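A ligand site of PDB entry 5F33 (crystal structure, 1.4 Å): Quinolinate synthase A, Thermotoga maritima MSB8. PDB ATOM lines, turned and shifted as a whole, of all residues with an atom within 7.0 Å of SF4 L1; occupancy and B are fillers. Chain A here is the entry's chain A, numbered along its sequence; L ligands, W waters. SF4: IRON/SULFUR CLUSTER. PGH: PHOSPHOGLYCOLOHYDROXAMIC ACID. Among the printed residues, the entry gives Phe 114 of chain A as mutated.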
ATOM      1  N   HIS A  26      15.120  19.451 -12.790  1.00  0.00           N
ATOM      2  CA  HIS A  26      15.374  19.259 -11.368  1.00  0.00           C
ATOM      3  C   HIS A  26      14.064  19.390 -10.578  1.00  0.00           C
ATOM      4  O   HIS A  26      13.143  20.137 -10.928  1.00  0.00           O
ATOM      5  CB  HIS A  26      16.480  20.189 -10.864  1.00  0.00           C
ATOM      6  CG  HIS A  26      16.909  19.892  -9.458  1.00  0.00           C
ATOM      7  ND1 HIS A  26      16.313  20.497  -8.385  1.00  0.00           N
ATOM      8  CD2 HIS A  26      17.793  19.009  -8.946  1.00  0.00           C
ATOM      9  CE1 HIS A  26      16.833  20.016  -7.277  1.00  0.00           C
ATOM     10  NE2 HIS A  26      17.731  19.104  -7.590  1.00  0.00           N
ATOM     11  N   TYR A  28      13.380  21.129  -8.092  1.00  0.00           N
ATOM     12  CA  TYR A  28      13.044  22.465  -7.585  1.00  0.00           C
ATOM     13  C   TYR A  28      12.447  23.342  -8.661  1.00  0.00           C
ATOM     14  O   TYR A  28      12.155  24.512  -8.418  1.00  0.00           O
ATOM     15  CB  TYR A  28      14.233  23.172  -6.960  1.00  0.00           C
ATOM     16  CG  TYR A  28      14.876  22.491  -5.766  1.00  0.00           C
ATOM     17  CD1 TYR A  28      14.225  21.479  -5.058  1.00  0.00           C
ATOM     18  CD2 TYR A  28      16.166  22.843  -5.368  1.00  0.00           C
ATOM     19  CE1 TYR A  28      14.818  20.884  -3.968  1.00  0.00           C
ATOM     20  CE2 TYR A  28      16.762  22.229  -4.267  1.00  0.00           C
ATOM     21  CZ  TYR A  28      16.091  21.237  -3.588  1.00  0.00           C
ATOM     22  OH  TYR A  28      16.709  20.664  -2.497  1.00  0.00           O
ATOM     23  N   VAL A  63      19.858  24.543 -12.784  1.00  0.00           N
ATOM     24  CA  VAL A  63      20.878  25.591 -12.727  1.00  0.00           C
ATOM     25  C   VAL A  63      22.120  25.196 -13.495  1.00  0.00           C
ATOM     26  O   VAL A  63      22.324  23.991 -13.823  1.00  0.00           O
ATOM     27  CB  VAL A  63      21.239  26.014 -11.322  1.00  0.00           C
ATOM     28  CG1 VAL A  63      20.044  26.669 -10.628  1.00  0.00           C
ATOM     29  CG2 VAL A  63      21.787  24.824 -10.525  1.00  0.00           C
ATOM     30  N   THR A  87      21.865  29.918 -11.727  1.00  0.00           N
ATOM     31  CA  THR A  87      23.101  29.399 -11.171  1.00  0.00           C
ATOM     32  C   THR A  87      22.923  29.139  -9.679  1.00  0.00           C
ATOM     33  O   THR A  87      21.889  29.473  -9.118  1.00  0.00           O
ATOM     34  CB  THR A  87      24.281  30.355 -11.421  1.00  0.00           C
ATOM     35  OG1 THR A  87      25.504  29.695 -11.087  1.00  0.00           O
ATOM     36  CG2 THR A  87      24.148  31.654 -10.642  1.00  0.00           C
ATOM     37  N   CYS A  88      23.888  28.496  -9.063  1.00  0.00           N
ATOM     38  CA  CYS A  88      23.873  28.308  -7.605  1.00  0.00           C
ATOM     39  C   CYS A  88      24.908  29.268  -6.978  1.00  0.00           C
ATOM     40  O   CYS A  88      26.085  29.128  -7.214  1.00  0.00           O
ATOM     41  CB  CYS A  88      24.210  26.871  -7.242  1.00  0.00           C
ATOM     42  SG  CYS A  88      24.362  26.616  -5.463  1.00  0.00           S
ATOM     43  N   PRO A  89      24.452  30.272  -6.215  1.00  0.00           N
ATOM     44  CA  PRO A  89      25.386  31.279  -5.673  1.00  0.00           C
ATOM     45  C   PRO A  89      26.505  30.730  -4.788  1.00  0.00           C
ATOM     46  O   PRO A  89      27.596  31.303  -4.771  1.00  0.00           O
ATOM     47  CB  PRO A  89      24.456  32.193  -4.882  1.00  0.00           C
ATOM     48  CG  PRO A  89      23.140  32.076  -5.584  1.00  0.00           C
ATOM     49  CD  PRO A  89      23.048  30.646  -5.977  1.00  0.00           C
ATOM     50  N   MET A  90      26.249  29.598  -4.143  1.00  0.00           N
ATOM     51  CA  MET A  90      27.237  28.928  -3.289  1.00  0.00           C
ATOM     52  C   MET A  90      28.550  28.587  -4.034  1.00  0.00           C
ATOM     53  O   MET A  90      29.624  28.582  -3.434  1.00  0.00           O
ATOM     54  CB  MET A  90      26.587  27.676  -2.681  1.00  0.00           C
ATOM     55  CG  MET A  90      27.385  26.919  -1.642  1.00  0.00           C
ATOM     56  SD  MET A  90      26.386  25.593  -0.929  1.00  0.00           S
ATOM     57  CE  MET A  90      26.153  24.475  -2.306  1.00  0.00           C
ATOM     58  N   ALA A  91      28.493  28.353  -5.329  1.00  0.00           N
ATOM     59  CA  ALA A  91      29.678  27.956  -6.101  1.00  0.00           C
ATOM     60  C   ALA A  91      30.765  29.028  -6.341  1.00  0.00           C
ATOM     61  O   ALA A  91      31.949  28.701  -6.355  1.00  0.00           O
ATOM     62  CB  ALA A  91      29.244  27.414  -7.436  1.00  0.00           C
ATOM     63  N   PHE A 114      31.096  18.886  -4.367  1.00  0.00           N
ATOM     64  CA  PHE A 114      29.662  18.838  -4.549  1.00  0.00           C
ATOM     65  C   PHE A 114      29.371  19.319  -5.972  1.00  0.00           C
ATOM     66  O   PHE A 114      30.066  20.172  -6.539  1.00  0.00           O
ATOM     67  CB  PHE A 114      29.040  19.708  -3.451  1.00  0.00           C
ATOM     68  CG  PHE A 114      27.539  19.756  -3.427  1.00  0.00           C
ATOM     69  CD1 PHE A 114      26.776  18.583  -3.400  1.00  0.00           C
ATOM     70  CD2 PHE A 114      26.879  20.985  -3.352  1.00  0.00           C
ATOM     71  CE1 PHE A 114      25.402  18.642  -3.353  1.00  0.00           C
ATOM     72  CE2 PHE A 114      25.489  21.046  -3.323  1.00  0.00           C
ATOM     73  CZ  PHE A 114      24.750  19.870  -3.319  1.00  0.00           C
ATOM     74  N   ASN A 116      27.219  21.347  -7.151  1.00  0.00           N
ATOM     75  CA  ASN A 116      27.060  22.786  -7.282  1.00  0.00           C
ATOM     76  C   ASN A 116      28.411  23.480  -7.123  1.00  0.00           C
ATOM     77  O   ASN A 116      28.759  24.008  -6.078  1.00  0.00           O
ATOM     78  CB  ASN A 116      25.977  23.309  -6.339  1.00  0.00           C
ATOM     79  CG  ASN A 116      24.583  22.818  -6.736  1.00  0.00           C
ATOM     80  OD1 ASN A 116      24.388  22.136  -7.777  1.00  0.00           O
ATOM     81  ND2 ASN A 116      23.605  23.131  -5.912  1.00  0.00           N
ATOM     82  N   ASP A 151      29.801  23.188   0.092  1.00  0.00           N
ATOM     83  CA  ASP A 151      28.785  23.245   1.170  1.00  0.00           C
ATOM     84  C   ASP A 151      29.325  22.689   2.490  1.00  0.00           C
ATOM     85  O   ASP A 151      29.608  21.503   2.592  1.00  0.00           O
ATOM     86  CB  ASP A 151      27.524  22.500   0.741  1.00  0.00           C
ATOM     87  CG  ASP A 151      26.360  22.769   1.646  1.00  0.00           C
ATOM     88  OD1 ASP A 151      26.343  22.234   2.756  1.00  0.00           O
ATOM     89  OD2 ASP A 151      25.442  23.491   1.262  1.00  0.00           O
ATOM     90  N   HIS A 174      27.482  27.639   2.101  1.00  0.00           N
ATOM     91  CA  HIS A 174      26.206  27.102   2.552  1.00  0.00           C
ATOM     92  C   HIS A 174      25.109  27.511   1.603  1.00  0.00           C
ATOM     93  O   HIS A 174      25.261  28.442   0.814  1.00  0.00           O
ATOM     94  CB  HIS A 174      25.876  27.618   3.966  1.00  0.00           C
ATOM     95  CG  HIS A 174      25.520  29.074   4.012  1.00  0.00           C
ATOM     96  ND1 HIS A 174      26.459  30.073   3.932  1.00  0.00           N
ATOM     97  CD2 HIS A 174      24.316  29.681   4.076  1.00  0.00           C
ATOM     98  CE1 HIS A 174      25.850  31.244   3.982  1.00  0.00           C
ATOM     99  NE2 HIS A 174      24.552  31.045   4.069  1.00  0.00           N
ATOM    100  N   CYS A 175      24.009  26.784   1.682  1.00  0.00           N
ATOM    101  CA  CYS A 175      22.837  27.034   0.845  1.00  0.00           C
ATOM    102  C   CYS A 175      21.880  27.846   1.695  1.00  0.00           C
ATOM    103  O   CYS A 175      21.353  27.307   2.670  1.00  0.00           O
ATOM    104  CB  CYS A 175      22.186  25.723   0.432  1.00  0.00           C
ATOM    105  SG  CYS A 175      20.539  26.013  -0.294  1.00  0.00           S
ATOM    106  N   PRO A 176      21.567  29.105   1.300  1.00  0.00           N
ATOM    107  CA  PRO A 176      20.616  29.903   2.098  1.00  0.00           C
ATOM    108  C   PRO A 176      19.207  29.301   2.180  1.00  0.00           C
ATOM    109  O   PRO A 176      18.503  29.492   3.151  1.00  0.00           O
ATOM    110  CB  PRO A 176      20.578  31.255   1.381  1.00  0.00           C
ATOM    111  CG  PRO A 176      21.129  31.009   0.023  1.00  0.00           C
ATOM    112  CD  PRO A 176      22.054  29.841   0.112  1.00  0.00           C
ATOM    113  N   VAL A 177      18.818  28.563   1.149  1.00  0.00           N
ATOM    114  CA  VAL A 177      17.479  28.024   1.069  1.00  0.00           C
ATOM    115  C   VAL A 177      17.237  27.000   2.196  1.00  0.00           C
ATOM    116  O   VAL A 177      16.142  26.941   2.763  1.00  0.00           O
ATOM    117  CB  VAL A 177      17.237  27.418  -0.360  1.00  0.00           C
ATOM    118  CG1 VAL A 177      15.832  26.860  -0.459  1.00  0.00           C
ATOM    119  CG2 VAL A 177      17.436  28.473  -1.449  1.00  0.00           C
ATOM    120  N   HIS A 178      18.269  26.256   2.562  1.00  0.00           N
ATOM    121  CA  HIS A 178      18.149  25.175   3.532  1.00  0.00           C
ATOM    122  C   HIS A 178      18.473  25.588   4.975  1.00  0.00           C
ATOM    123  O   HIS A 178      18.530  24.733   5.881  1.00  0.00           O
ATOM    124  CB  HIS A 178      19.032  24.012   3.088  1.00  0.00           C
ATOM    125  CG  HIS A 178      18.443  23.227   1.967  1.00  0.00           C
ATOM    126  ND1 HIS A 178      18.737  23.478   0.645  1.00  0.00           N
ATOM    127  CD2 HIS A 178      17.504  22.252   1.972  1.00  0.00           C
ATOM    128  CE1 HIS A 178      18.036  22.648  -0.112  1.00  0.00           C
ATOM    129  NE2 HIS A 178      17.298  21.881   0.670  1.00  0.00           N
ATOM    130  N   HIS A 200      16.932  17.893   4.179  1.00  0.00           N
ATOM    131  CA  HIS A 200      18.078  17.781   3.286  1.00  0.00           C
ATOM    132  C   HIS A 200      19.373  17.844   4.064  1.00  0.00           C
ATOM    133  O   HIS A 200      19.425  18.549   5.055  1.00  0.00           O
ATOM    134  CB  HIS A 200      18.021  18.942   2.309  1.00  0.00           C
ATOM    135  CG  HIS A 200      18.760  18.686   1.044  1.00  0.00           C
ATOM    136  ND1 HIS A 200      20.123  18.855   0.951  1.00  0.00           N
ATOM    137  CD2 HIS A 200      18.350  18.171  -0.137  1.00  0.00           C
ATOM    138  CE1 HIS A 200      20.511  18.497  -0.255  1.00  0.00           C
ATOM    139  NE2 HIS A 200      19.460  18.079  -0.923  1.00  0.00           N
ATOM    140  N   GLU A 202      21.926  19.509   3.394  1.00  0.00           N
ATOM    141  CA  GLU A 202      22.392  20.901   3.303  1.00  0.00           C
ATOM    142  C   GLU A 202      21.847  21.745   4.467  1.00  0.00           C
ATOM    143  O   GLU A 202      22.288  22.879   4.658  1.00  0.00           O
ATOM    144  CB  GLU A 202      21.970  21.557   1.964  1.00  0.00           C
ATOM    145  CG  GLU A 202      22.783  21.078   0.762  1.00  0.00           C
ATOM    146  CD  GLU A 202      22.158  21.458  -0.561  1.00  0.00           C
ATOM    147  OE1 GLU A 202      21.435  22.478  -0.656  1.00  0.00           O
ATOM    148  OE2 GLU A 202      22.349  20.713  -1.524  1.00  0.00           O
ATOM    149  N   THR A 236      13.117  21.104   2.633  1.00  0.00           N
ATOM    150  CA  THR A 236      13.897  21.425   1.430  1.00  0.00           C
ATOM    151  C   THR A 236      13.135  22.479   0.663  1.00  0.00           C
ATOM    152  O   THR A 236      12.154  23.044   1.162  1.00  0.00           O
ATOM    153  CB  THR A 236      14.235  20.158   0.589  1.00  0.00           C
ATOM    154  OG1 THR A 236      15.272  20.487  -0.327  1.00  0.00           O
ATOM    155  CG2 THR A 236      13.003  19.634  -0.176  1.00  0.00           C
ATOM    156  N   GLU A 237      13.625  22.803  -0.536  1.00  0.00           N
ATOM    157  CA  GLU A 237      13.061  23.841  -1.381  1.00  0.00           C
ATOM    158  C   GLU A 237      11.634  23.430  -1.809  1.00  0.00           C
ATOM    159  O   GLU A 237      11.350  22.249  -2.010  1.00  0.00           O
ATOM    160  CB  GLU A 237      13.976  24.053  -2.586  1.00  0.00           C
ATOM    161  CG  GLU A 237      13.872  25.395  -3.256  1.00  0.00           C
ATOM    162  CD  GLU A 237      12.779  25.535  -4.284  1.00  0.00           C
ATOM    163  OE1 GLU A 237      12.154  24.548  -4.711  1.00  0.00           O
ATOM    164  OE2 GLU A 237      12.548  26.681  -4.715  1.00  0.00           O
ATOM    165  N   VAL A 260      12.454  29.114  -0.970  1.00  0.00           N
ATOM    166  CA  VAL A 260      12.424  29.283  -2.439  1.00  0.00           C
ATOM    167  C   VAL A 260      13.835  29.545  -2.911  1.00  0.00           C
ATOM    168  O   VAL A 260      14.506  30.402  -2.373  1.00  0.00           O
ATOM    169  CB  VAL A 260      11.485  30.421  -2.906  1.00  0.00           C
ATOM    170  CG1 VAL A 260      11.491  30.577  -4.414  1.00  0.00           C
ATOM    171  CG2 VAL A 260      10.067  30.192  -2.403  1.00  0.00           C
ATOM    172  N   CYS A 261      14.275  28.808  -3.928  1.00  0.00           N
ATOM    173  CA  CYS A 261      15.550  29.078  -4.602  1.00  0.00           C
ATOM    174  C   CYS A 261      15.213  29.960  -5.782  1.00  0.00           C
ATOM    175  O   CYS A 261      14.642  29.479  -6.780  1.00  0.00           O
ATOM    176  CB  CYS A 261      16.211  27.814  -5.060  1.00  0.00           C
ATOM    177  SG  CYS A 261      17.747  28.142  -5.944  1.00  0.00           S
ATOM    178  N   VAL A 262      15.521  31.252  -5.641  1.00  0.00           N
ATOM    179  CA  VAL A 262      15.243  32.227  -6.703  1.00  0.00           C
ATOM    180  C   VAL A 262      15.830  31.768  -8.057  1.00  0.00           C
ATOM    181  O   VAL A 262      15.193  31.885  -9.093  1.00  0.00           O
ATOM    182  CB  VAL A 262      15.747  33.632  -6.273  1.00  0.00           C
ATOM    183  CG1 VAL A 262      15.815  34.604  -7.435  1.00  0.00           C
ATOM    184  CG2 VAL A 262      14.834  34.178  -5.178  1.00  0.00           C
ATOM    185  N   ASN A 263      17.051  31.253  -8.043  1.00  0.00           N
ATOM    186  CA  ASN A 263      17.680  30.806  -9.268  1.00  0.00           C
ATOM    187  C   ASN A 263      16.915  29.680  -9.927  1.00  0.00           C
ATOM    188  O   ASN A 263      16.731  29.706 -11.154  1.00  0.00           O
ATOM    189  CB  ASN A 263      19.139  30.455  -9.053  1.00  0.00           C
ATOM    190  CG  ASN A 263      20.040  31.642  -9.238  1.00  0.00           C
ATOM    191  OD1 ASN A 263      20.338  32.037 -10.375  1.00  0.00           O
ATOM    192  ND2 ASN A 263      20.418  32.276  -8.130  1.00  0.00           N
ATOM    193  N   MET A 264      16.427  28.731  -9.144  1.00  0.00           N
ATOM    194  CA  MET A 264      15.616  27.650  -9.723  1.00  0.00           C
ATOM    195  C   MET A 264      14.306  28.148 -10.302  1.00  0.00           C
ATOM    196  O   MET A 264      13.801  27.548 -11.245  1.00  0.00           O
ATOM    197  CB  MET A 264      15.347  26.573  -8.666  1.00  0.00           C
ATOM    198  CG  MET A 264      16.570  25.729  -8.331  1.00  0.00           C
ATOM    199  SD  MET A 264      16.857  24.516  -9.628  1.00  0.00           S
ATOM    200  CE  MET A 264      18.147  23.575  -8.799  1.00  0.00           C
HETATM  201 FE1  SF4 L   1      20.611  26.016  -2.569  1.00  0.00          FE
HETATM  202 FE2  SF4 L   1      19.524  26.872  -4.964  1.00  0.00          FE
HETATM  203 FE3  SF4 L   1      20.452  24.089  -4.516  1.00  0.00          FE
HETATM  204 FE4  SF4 L   1      22.196  26.312  -4.788  1.00  0.00          FE
HETATM  205  S1  SF4 L   1      20.793  25.637  -6.401  1.00  0.00           S
HETATM  206  S2  SF4 L   1      22.249  24.574  -3.178  1.00  0.00           S
HETATM  207  S3  SF4 L   1      21.046  28.033  -3.676  1.00  0.00           S
HETATM  208  S4  SF4 L   1      18.688  25.323  -3.503  1.00  0.00           S
HETATM  209  C1  PGH L   2      20.042  21.153  -4.094  1.00  0.00           C
HETATM  210  C2  PGH L   2      19.552  19.776  -3.707  1.00  0.00           C
HETATM  211  N2  PGH L   2      20.419  21.338  -5.350  1.00  0.00           N
HETATM  212  O2  PGH L   2      20.747  22.595  -5.836  1.00  0.00           O
HETATM  213  O1  PGH L   2      19.987  22.058  -3.248  1.00  0.00           O
HETATM  214  O1P PGH L   2      20.198  18.653  -4.296  1.00  0.00           O
HETATM  215  O2P PGH L   2      19.060  16.660  -3.342  1.00  0.00           O
HETATM  216  O3P PGH L   2      18.306  17.537  -5.601  1.00  0.00           O
HETATM  217  O4P PGH L   2      20.547  16.544  -5.408  1.00  0.00           O
HETATM  218  P   PGH L   2      19.453  17.257  -4.655  1.00  0.00           P
HETATM  219  O   HOH W   1      23.668  29.551  -2.827  1.00  0.00           O
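Water W1 lies within hydrogen-bond range of N of Met 90 (2.9 Å) and S3 of SF4 L1 (3.1 Å).
A sulfur (S2) of SF4 L1 sits close to the side-chain carboxylate (OE1) of Glu 202, at 3.4 Å.
Residues that only touch SF4 L1: Tyr 28 and Val 177.
Hydrophobic or aromatic side chains that line SF4 L1: Tyr 28 and Val 177.
Of the 25 residues printed, 7 come within 4 Å of SF4 L1.
The side-chain sulfur of Cys 175 is bound to an iron atom (FE1) of SF4 L1 (2.3 Å).
SG of Cys 88 binds FE4 of SF4 L1.
SG of Cys 261 binds FE2 of SF4 L1 (2.4 Å).
The side-chain amide nitrogen (ND2) of Asn 116 sits close to a sulfur (S2) of SF4 L1.
The side-chain amide nitrogen (ND2) of Asn 116 lies close to an oxygen (O2) of PGH L2 (2.9 Å).
A ring nitrogen (NE2) of His 26 lies within hydrogen-bond range of an oxygen (O3P) of PGH L2 (2.6 Å).
A ring nitrogen (NE2) of His 200 lies within hydrogen-bond range of an oxygen (O2P) of PGH L2 (2.8 Å).
An iron atom (FE3) of SF4 L1 is bound by an oxygen (O2) of PGH L2 (2.0 Å).
The backbone NH of Cys 175 sits at hydrogen-bond distance from the side-chain sulfur of Met 90, 3.7 Å away.
The side-chain sulfur (SG) of Cys 175 lies close to a ring nitrogen (ND1) of His 178, at 3.2 Å.
The backbone NH of Met 90 lies close to the side-chain sulfur of Cys 88 (3.8 Å).
N of Met 264 lies close to SG of Cys 261.
The side-chain carboxylate (OE1) of Glu 202 lies within hydrogen-bond range of a ring nitrogen (ND1) of His 178, at 3.2 Å.
N of Glu 202 is in hydrogen-bond range of ND1 of His 200.
A ring nitrogen (NE2) of His 178 sits close to the side-chain hydroxyl (OH) of Tyr 28, 3.4 Å away.
The side-chain hydroxyl (OG1) of Thr 236 sits at hydrogen-bond distance from the side-chain hydroxyl (OH) of Tyr 28 (2.6 Å).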
